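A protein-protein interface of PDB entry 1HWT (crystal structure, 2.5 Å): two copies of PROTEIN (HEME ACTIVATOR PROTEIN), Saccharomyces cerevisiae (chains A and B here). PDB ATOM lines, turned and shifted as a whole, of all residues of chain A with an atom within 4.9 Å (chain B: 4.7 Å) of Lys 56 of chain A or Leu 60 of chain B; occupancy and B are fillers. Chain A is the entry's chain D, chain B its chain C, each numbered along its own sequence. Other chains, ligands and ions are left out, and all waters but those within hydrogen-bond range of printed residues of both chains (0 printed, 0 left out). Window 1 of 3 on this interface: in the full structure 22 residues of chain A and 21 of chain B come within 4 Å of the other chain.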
ATOM      1  N   GLU A  51      14.756   3.725 -25.130  1.00  0.00           N
ATOM      2  CA  GLU A  51      14.045   2.837 -24.212  1.00  0.00           C
ATOM      3  C   GLU A  51      13.884   3.543 -22.874  1.00  0.00           C
ATOM      4  O   GLU A  51      12.798   3.599 -22.307  1.00  0.00           O
ATOM      5  CB  GLU A  51      14.843   1.545 -24.001  1.00  0.00           C
ATOM      6  CG  GLU A  51      14.008   0.279 -23.998  1.00  0.00           C
ATOM      7  CD  GLU A  51      14.152  -0.488 -25.294  1.00  0.00           C
ATOM      8  OE1 GLU A  51      15.225  -1.121 -25.470  1.00  0.00           O
ATOM      9  OE2 GLU A  51      13.206  -0.452 -26.138  1.00  0.00           O
ATOM     10  N   LYS A  52      14.995   4.064 -22.368  1.00  0.00           N
ATOM     11  CA  LYS A  52      15.022   4.787 -21.098  1.00  0.00           C
ATOM     12  C   LYS A  52      13.918   5.841 -21.100  1.00  0.00           C
ATOM     13  O   LYS A  52      13.218   6.040 -20.106  1.00  0.00           O
ATOM     14  CB  LYS A  52      16.388   5.457 -20.934  1.00  0.00           C
ATOM     15  CG  LYS A  52      16.574   6.206 -19.645  1.00  0.00           C
ATOM     16  CD  LYS A  52      18.019   6.098 -19.169  1.00  0.00           C
ATOM     17  CE  LYS A  52      18.236   6.843 -17.850  1.00  0.00           C
ATOM     18  NZ  LYS A  52      17.797   8.278 -17.946  1.00  0.00           N
ATOM     19  N   GLU A  53      13.773   6.510 -22.237  1.00  0.00           N
ATOM     20  CA  GLU A  53      12.781   7.559 -22.412  1.00  0.00           C
ATOM     21  C   GLU A  53      11.351   7.038 -22.404  1.00  0.00           C
ATOM     22  O   GLU A  53      10.512   7.511 -21.642  1.00  0.00           O
ATOM     23  CB  GLU A  53      13.048   8.302 -23.712  1.00  0.00           C
ATOM     24  CG  GLU A  53      13.401   9.748 -23.518  1.00  0.00           C
ATOM     25  CD  GLU A  53      14.730  10.111 -24.129  1.00  0.00           C
ATOM     26  OE1 GLU A  53      15.765   9.911 -23.459  1.00  0.00           O
ATOM     27  OE2 GLU A  53      14.738  10.598 -25.280  1.00  0.00           O
ATOM     28  N   LEU A  54      11.059   6.064 -23.254  1.00  0.00           N
ATOM     29  CA  LEU A  54       9.717   5.498 -23.305  1.00  0.00           C
ATOM     30  C   LEU A  54       9.253   5.036 -21.933  1.00  0.00           C
ATOM     31  O   LEU A  54       8.140   5.346 -21.521  1.00  0.00           O
ATOM     32  CB  LEU A  54       9.690   4.317 -24.260  1.00  0.00           C
ATOM     33  CG  LEU A  54       8.488   4.162 -25.188  1.00  0.00           C
ATOM     34  CD1 LEU A  54       8.388   5.356 -26.133  1.00  0.00           C
ATOM     35  CD2 LEU A  54       8.646   2.860 -25.958  1.00  0.00           C
ATOM     36  N   LEU A  55      10.119   4.296 -21.236  1.00  0.00           N
ATOM     37  CA  LEU A  55       9.836   3.752 -19.902  1.00  0.00           C
ATOM     38  C   LEU A  55       9.617   4.850 -18.867  1.00  0.00           C
ATOM     39  O   LEU A  55       8.742   4.754 -18.003  1.00  0.00           O
ATOM     40  CB  LEU A  55      11.003   2.876 -19.449  1.00  0.00           C
ATOM     41  CG  LEU A  55      10.794   1.383 -19.199  1.00  0.00           C
ATOM     42  CD1 LEU A  55       9.393   0.939 -19.622  1.00  0.00           C
ATOM     43  CD2 LEU A  55      11.862   0.628 -19.970  1.00  0.00           C
ATOM     44  N   LYS A  56      10.445   5.886 -18.953  1.00  0.00           N
ATOM     45  CA  LYS A  56      10.365   7.018 -18.039  1.00  0.00           C
ATOM     46  C   LYS A  56       9.044   7.746 -18.241  1.00  0.00           C
ATOM     47  O   LYS A  56       8.417   8.199 -17.283  1.00  0.00           O
ATOM     48  CB  LYS A  56      11.526   7.965 -18.293  1.00  0.00           C
ATOM     49  CG  LYS A  56      11.507   9.214 -17.441  1.00  0.00           C
ATOM     50  CD  LYS A  56      12.293  10.328 -18.114  1.00  0.00           C
ATOM     51  CE  LYS A  56      13.754   9.956 -18.269  1.00  0.00           C
ATOM     52  NZ  LYS A  56      14.565  11.143 -18.649  1.00  0.00           N
ATOM     53  N   ASP A  57       8.619   7.848 -19.491  1.00  0.00           N
ATOM     54  CA  ASP A  57       7.366   8.499 -19.803  1.00  0.00           C
ATOM     55  C   ASP A  57       6.218   7.683 -19.214  1.00  0.00           C
ATOM     56  O   ASP A  57       5.251   8.241 -18.688  1.00  0.00           O
ATOM     57  CB  ASP A  57       7.202   8.598 -21.313  1.00  0.00           C
ATOM     58  CG  ASP A  57       7.779   9.864 -21.870  1.00  0.00           C
ATOM     59  OD1 ASP A  57       8.146  10.741 -21.079  1.00  0.00           O
ATOM     60  OD2 ASP A  57       7.876   9.988 -23.100  1.00  0.00           O
ATOM     61  N   ASN A  58       6.325   6.361 -19.314  1.00  0.00           N
ATOM     62  CA  ASN A  58       5.291   5.464 -18.803  1.00  0.00           C
ATOM     63  C   ASN A  58       5.226   5.579 -17.302  1.00  0.00           C
ATOM     64  O   ASN A  58       4.148   5.558 -16.718  1.00  0.00           O
ATOM     65  CB  ASN A  58       5.596   4.008 -19.184  1.00  0.00           C
ATOM     66  CG  ASN A  58       4.624   3.001 -18.555  1.00  0.00           C
ATOM     67  OD1 ASN A  58       4.887   2.421 -17.499  1.00  0.00           O
ATOM     68  ND2 ASN A  58       3.506   2.782 -19.219  1.00  0.00           N
ATOM     69  N   GLU A  59       6.387   5.695 -16.673  1.00  0.00           N
ATOM     70  CA  GLU A  59       6.452   5.792 -15.221  1.00  0.00           C
ATOM     71  C   GLU A  59       5.856   7.075 -14.649  1.00  0.00           C
ATOM     72  O   GLU A  59       5.214   7.049 -13.596  1.00  0.00           O
ATOM     73  CB  GLU A  59       7.898   5.644 -14.749  1.00  0.00           C
ATOM     74  CG  GLU A  59       8.013   5.279 -13.282  1.00  0.00           C
ATOM     75  CD  GLU A  59       9.422   4.933 -12.865  1.00  0.00           C
ATOM     76  OE1 GLU A  59      10.361   5.103 -13.672  1.00  0.00           O
ATOM     77  OE2 GLU A  59       9.594   4.490 -11.719  1.00  0.00           O
ATOM     78  N   LEU A  60       6.087   8.202 -15.322  1.00  0.00           N
ATOM     79  CA  LEU A  60       5.546   9.464 -14.841  1.00  0.00           C
ATOM     80  C   LEU A  60       4.029   9.346 -14.984  1.00  0.00           C
ATOM     81  O   LEU A  60       3.283   9.707 -14.081  1.00  0.00           O
ATOM     82  CB  LEU A  60       6.083  10.687 -15.658  1.00  0.00           C
ATOM     83  CG  LEU A  60       7.536  10.952 -15.341  1.00  0.00           C
ATOM     84  N   LEU A  63       2.748   6.780 -12.341  1.00  0.00           N
ATOM     85  CA  LEU A  63       2.989   7.297 -11.000  1.00  0.00           C
ATOM     86  C   LEU A  63       1.994   8.415 -10.695  1.00  0.00           C
ATOM     87  O   LEU A  63       1.560   8.561  -9.557  1.00  0.00           O
ATOM     88  CB  LEU A  63       4.424   7.826 -10.872  1.00  0.00           C
ATOM     89  CG  LEU A  63       5.529   6.846 -10.468  1.00  0.00           C
ATOM     90  CD1 LEU A  63       6.866   7.505 -10.647  1.00  0.00           C
ATOM     91  CD2 LEU A  63       5.352   6.409  -9.031  1.00  0.00           C
ATOM     92  N   GLU B  53      14.428  16.353 -20.248  1.00  0.00           N
ATOM     93  CA  GLU B  53      14.520  15.032 -19.651  1.00  0.00           C
ATOM     94  C   GLU B  53      15.166  15.096 -18.282  1.00  0.00           C
ATOM     95  O   GLU B  53      15.034  14.174 -17.482  1.00  0.00           O
ATOM     96  CB  GLU B  53      15.319  14.100 -20.560  1.00  0.00           C
ATOM     97  CG  GLU B  53      14.599  13.735 -21.842  1.00  0.00           C
ATOM     98  CD  GLU B  53      13.191  13.226 -21.587  1.00  0.00           C
ATOM     99  OE1 GLU B  53      13.025  12.231 -20.847  1.00  0.00           O
ATOM    100  OE2 GLU B  53      12.236  13.816 -22.126  1.00  0.00           O
ATOM    101  N   LYS B  56      12.353  15.895 -16.037  1.00  0.00           N
ATOM    102  CA  LYS B  56      11.522  14.700 -15.936  1.00  0.00           C
ATOM    103  C   LYS B  56      12.137  13.807 -14.878  1.00  0.00           C
ATOM    104  O   LYS B  56      11.444  13.286 -14.023  1.00  0.00           O
ATOM    105  CB  LYS B  56      11.483  13.967 -17.269  1.00  0.00           C
ATOM    106  CG  LYS B  56      10.226  14.213 -18.053  1.00  0.00           C
ATOM    107  CD  LYS B  56      10.500  14.988 -19.301  1.00  0.00           C
ATOM    108  CE  LYS B  56       9.730  14.425 -20.495  1.00  0.00           C
ATOM    109  NZ  LYS B  56       9.959  12.961 -20.713  1.00  0.00           N
ATOM    110  N   ASP B  57      13.451  13.646 -14.934  1.00  0.00           N
ATOM    111  CA  ASP B  57      14.159  12.828 -13.958  1.00  0.00           C
ATOM    112  C   ASP B  57      13.801  13.255 -12.530  1.00  0.00           C
ATOM    113  O   ASP B  57      13.467  12.426 -11.676  1.00  0.00           O
ATOM    114  CB  ASP B  57      15.674  12.969 -14.153  1.00  0.00           C
ATOM    115  CG  ASP B  57      16.204  12.116 -15.279  1.00  0.00           C
ATOM    116  OD1 ASP B  57      15.394  11.606 -16.077  1.00  0.00           O
ATOM    117  OD2 ASP B  57      17.435  11.956 -15.369  1.00  0.00           O
ATOM    118  N   ASN B  58      13.877  14.557 -12.279  1.00  0.00           N
ATOM    119  CA  ASN B  58      13.579  15.112 -10.966  1.00  0.00           C
ATOM    120  C   ASN B  58      12.113  15.000 -10.572  1.00  0.00           C
ATOM    121  O   ASN B  58      11.790  14.709  -9.425  1.00  0.00           O
ATOM    122  CB  ASN B  58      14.005  16.573 -10.923  1.00  0.00           C
ATOM    123  CG  ASN B  58      14.617  16.953  -9.590  1.00  0.00           C
ATOM    124  OD1 ASN B  58      15.579  16.307  -9.131  1.00  0.00           O
ATOM    125  ND2 ASN B  58      14.058  18.003  -8.942  1.00  0.00           N
ATOM    126  N   GLU B  59      11.219  15.236 -11.522  1.00  0.00           N
ATOM    127  CA  GLU B  59       9.796  15.155 -11.238  1.00  0.00           C
ATOM    128  C   GLU B  59       9.459  13.717 -10.905  1.00  0.00           C
ATOM    129  O   GLU B  59       8.599  13.444 -10.062  1.00  0.00           O
ATOM    130  CB  GLU B  59       8.977  15.624 -12.450  1.00  0.00           C
ATOM    131  CG  GLU B  59       8.625  17.130 -12.450  1.00  0.00           C
ATOM    132  CD  GLU B  59       9.589  17.981 -11.586  1.00  0.00           C
ATOM    133  OE1 GLU B  59      10.677  18.376 -12.102  1.00  0.00           O
ATOM    134  OE2 GLU B  59       9.256  18.257 -10.397  1.00  0.00           O
ATOM    135  N   LEU B  60      10.141  12.792 -11.568  1.00  0.00           N
ATOM    136  CA  LEU B  60       9.927  11.366 -11.348  1.00  0.00           C
ATOM    137  C   LEU B  60      10.321  11.016  -9.914  1.00  0.00           C
ATOM    138  O   LEU B  60       9.568  10.365  -9.189  1.00  0.00           O
ATOM    139  CB  LEU B  60      10.771  10.572 -12.341  1.00  0.00           C
ATOM    140  CG  LEU B  60      10.154   9.309 -12.915  1.00  0.00           C
ATOM    141  CD1 LEU B  60      10.914   8.903 -14.156  1.00  0.00           C
ATOM    142  CD2 LEU B  60      10.222   8.217 -11.880  1.00  0.00           C
ATOM    143  N   LYS B  61      11.509  11.453  -9.518  1.00  0.00           N
ATOM    144  CA  LYS B  61      11.992  11.205  -8.175  1.00  0.00           C
ATOM    145  C   LYS B  61      10.981  11.729  -7.165  1.00  0.00           C
ATOM    146  O   LYS B  61      10.611  11.035  -6.226  1.00  0.00           O
ATOM    147  CB  LYS B  61      13.340  11.899  -7.972  1.00  0.00           C
ATOM    148  CG  LYS B  61      13.665  12.183  -6.514  1.00  0.00           C
ATOM    149  CD  LYS B  61      14.891  13.071  -6.388  1.00  0.00           C
ATOM    150  CE  LYS B  61      15.260  13.273  -4.934  1.00  0.00           C
ATOM    151  NZ  LYS B  61      16.742  13.226  -4.746  1.00  0.00           N
ATOM    152  N   LYS B  62      10.526  12.960  -7.363  1.00  0.00           N
ATOM    153  CA  LYS B  62       9.560  13.574  -6.454  1.00  0.00           C
ATOM    154  C   LYS B  62       8.235  12.832  -6.408  1.00  0.00           C
ATOM    155  O   LYS B  62       7.551  12.827  -5.380  1.00  0.00           O
ATOM    156  CB  LYS B  62       9.324  15.032  -6.848  1.00  0.00           C
ATOM    157  CG  LYS B  62      10.602  15.867  -6.871  1.00  0.00           C
ATOM    158  CD  LYS B  62      10.290  17.341  -6.745  1.00  0.00           C
ATOM    159  CE  LYS B  62      11.568  18.182  -6.725  1.00  0.00           C
ATOM    160  NZ  LYS B  62      11.634  19.207  -7.838  1.00  0.00           N
ATOM    161  N   LEU B  63       7.867  12.205  -7.514  1.00  0.00           N
ATOM    162  CA  LEU B  63       6.624  11.450  -7.565  1.00  0.00           C
ATOM    163  C   LEU B  63       6.743  10.176  -6.744  1.00  0.00           C
ATOM    164  O   LEU B  63       5.879   9.869  -5.917  1.00  0.00           O
ATOM    165  CB  LEU B  63       6.292  11.071  -8.999  1.00  0.00           C
ATOM    166  CG  LEU B  63       5.542  12.135  -9.782  1.00  0.00           C
ATOM    167  CD1 LEU B  63       5.497  11.749 -11.242  1.00  0.00           C
ATOM    168  CD2 LEU B  63       4.143  12.286  -9.206  1.00  0.00           C
ATOM    169  N   ARG B  64       7.815   9.426  -6.983  1.00  0.00           N
ATOM    170  CA  ARG B  64       8.020   8.174  -6.269  1.00  0.00           C
ATOM    171  C   ARG B  64       8.025   8.461  -4.777  1.00  0.00           C
ATOM    172  O   ARG B  64       7.581   7.632  -3.979  1.00  0.00           O
ATOM    173  CB  ARG B  64       9.338   7.519  -6.700  1.00  0.00           C
ATOM    174  CG  ARG B  64       9.356   6.006  -6.487  1.00  0.00           C
ATOM    175  CD  ARG B  64      10.778   5.473  -6.473  1.00  0.00           C
ATOM    176  NE  ARG B  64      11.346   5.492  -7.813  1.00  0.00           N
ATOM    177  CZ  ARG B  64      10.941   4.687  -8.785  1.00  0.00           C
ATOM    178  NH1 ARG B  64       9.973   3.816  -8.531  1.00  0.00           N
ATOM    179  NH2 ARG B  64      11.505   4.743  -9.993  1.00  0.00           N
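The guanidinium group (NH2) of Arg 64 of chain B lies within salt-bridge range of the side-chain carboxylate (OE2) of Glu 59 of chain A (2.6 Å). NZ of Lys 56 of chain B is in salt-bridge range of OD1 of Asp 57 of chain A, 2.9 Å away. The side-chain amino group of Lys 56 of chain A lies within salt-bridge range of the side-chain carboxylate of Glu 53 of chain B, 2.9 Å away. NZ of Lys 56 of chain A is in salt-bridge range of OD1 of Asp 57 of chain B.
The side-chain carboxylate (OE2) of Glu 53 of chain B is in salt-bridge range of the side-chain amino group (NZ) of Lys 56 of chain B (2.8 Å).
Among the printed residues, pairs that only touch across the chains: Glu 53 of chain A with Glu 53 of chain B (3.7 Å), Lys 56 of chain A with Lys 56 of chain B (3.8 Å), Lys 56 of chain A with Leu 60 of chain B (3.4 Å), Glu 59 of chain A with Leu 60 of chain B (3.5 Å), Leu 60 of chain A with Leu 60 of chain B (3.9 Å), Leu 63 of chain A with Leu 60 of chain B (3.6 Å) and Leu 63 of chain A with Leu 63 of chain B (3.97 Å).
Glu 53 of chain B touches its own counterpart, Glu 53 of chain A. Lys 56 of chain A touches Glu 53 of chain B, but with the chains exchanged Glu 53 of chain A does not touch Lys 56 of chain B (5.5 Å). Lys 56 of chain A touches Leu 60 of chain B, but with the chains exchanged Leu 60 of chain A does not touch Lys 56 of chain B (4.7 Å). Glu 59 of chain A touches Leu 60 of chain B, but with the chains exchanged Leu 60 of chain A does not touch Glu 59 of chain B (5.6 Å). Positions printed for both chains: 53, 56, 57, 58, 59, 60 and 63. Of the 11 pairs that touch across the chains among the printed residues, 6 have their exchanged pair printed and touching as well.
Printed residues of chain B within 4 Å of Glu 53 of chain A: Glu 53. Printed residues of chain B within 4 Å of Lys 56 of chain A: Glu 53, Lys 56, Asp 57 and Leu 60. Of the printed residues of chain B, Glu 59 of chain A touches Leu 60 and Arg 64. Of the printed residues of chain A, Glu 53 of chain B touches Glu 53 (3.7 Å) and Lys 56 (2.9 Å). Printed residues of chain A within 4 Å of Asp 57 of chain B: Lys 56 (2.7 Å). Of chain A, only Lys 56, Glu 59, Leu 60 and Leu 63 come within 4 Å of Leu 60 of chain B. Of the printed residues of chain A, Arg 64 of chain B touches Glu 59. The nearest printed residue of chain B that does not touch Asp 57 of chain A is Glu 53 of chain B (5.1 Å).
Hydrophobic or aromatic side chains of chain A that line the printed part of chain B: Leu 60 and Leu 63. Hydrophobic or aromatic side chains of chain B that line the printed part of chain A: Leu 60 and Leu 63.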
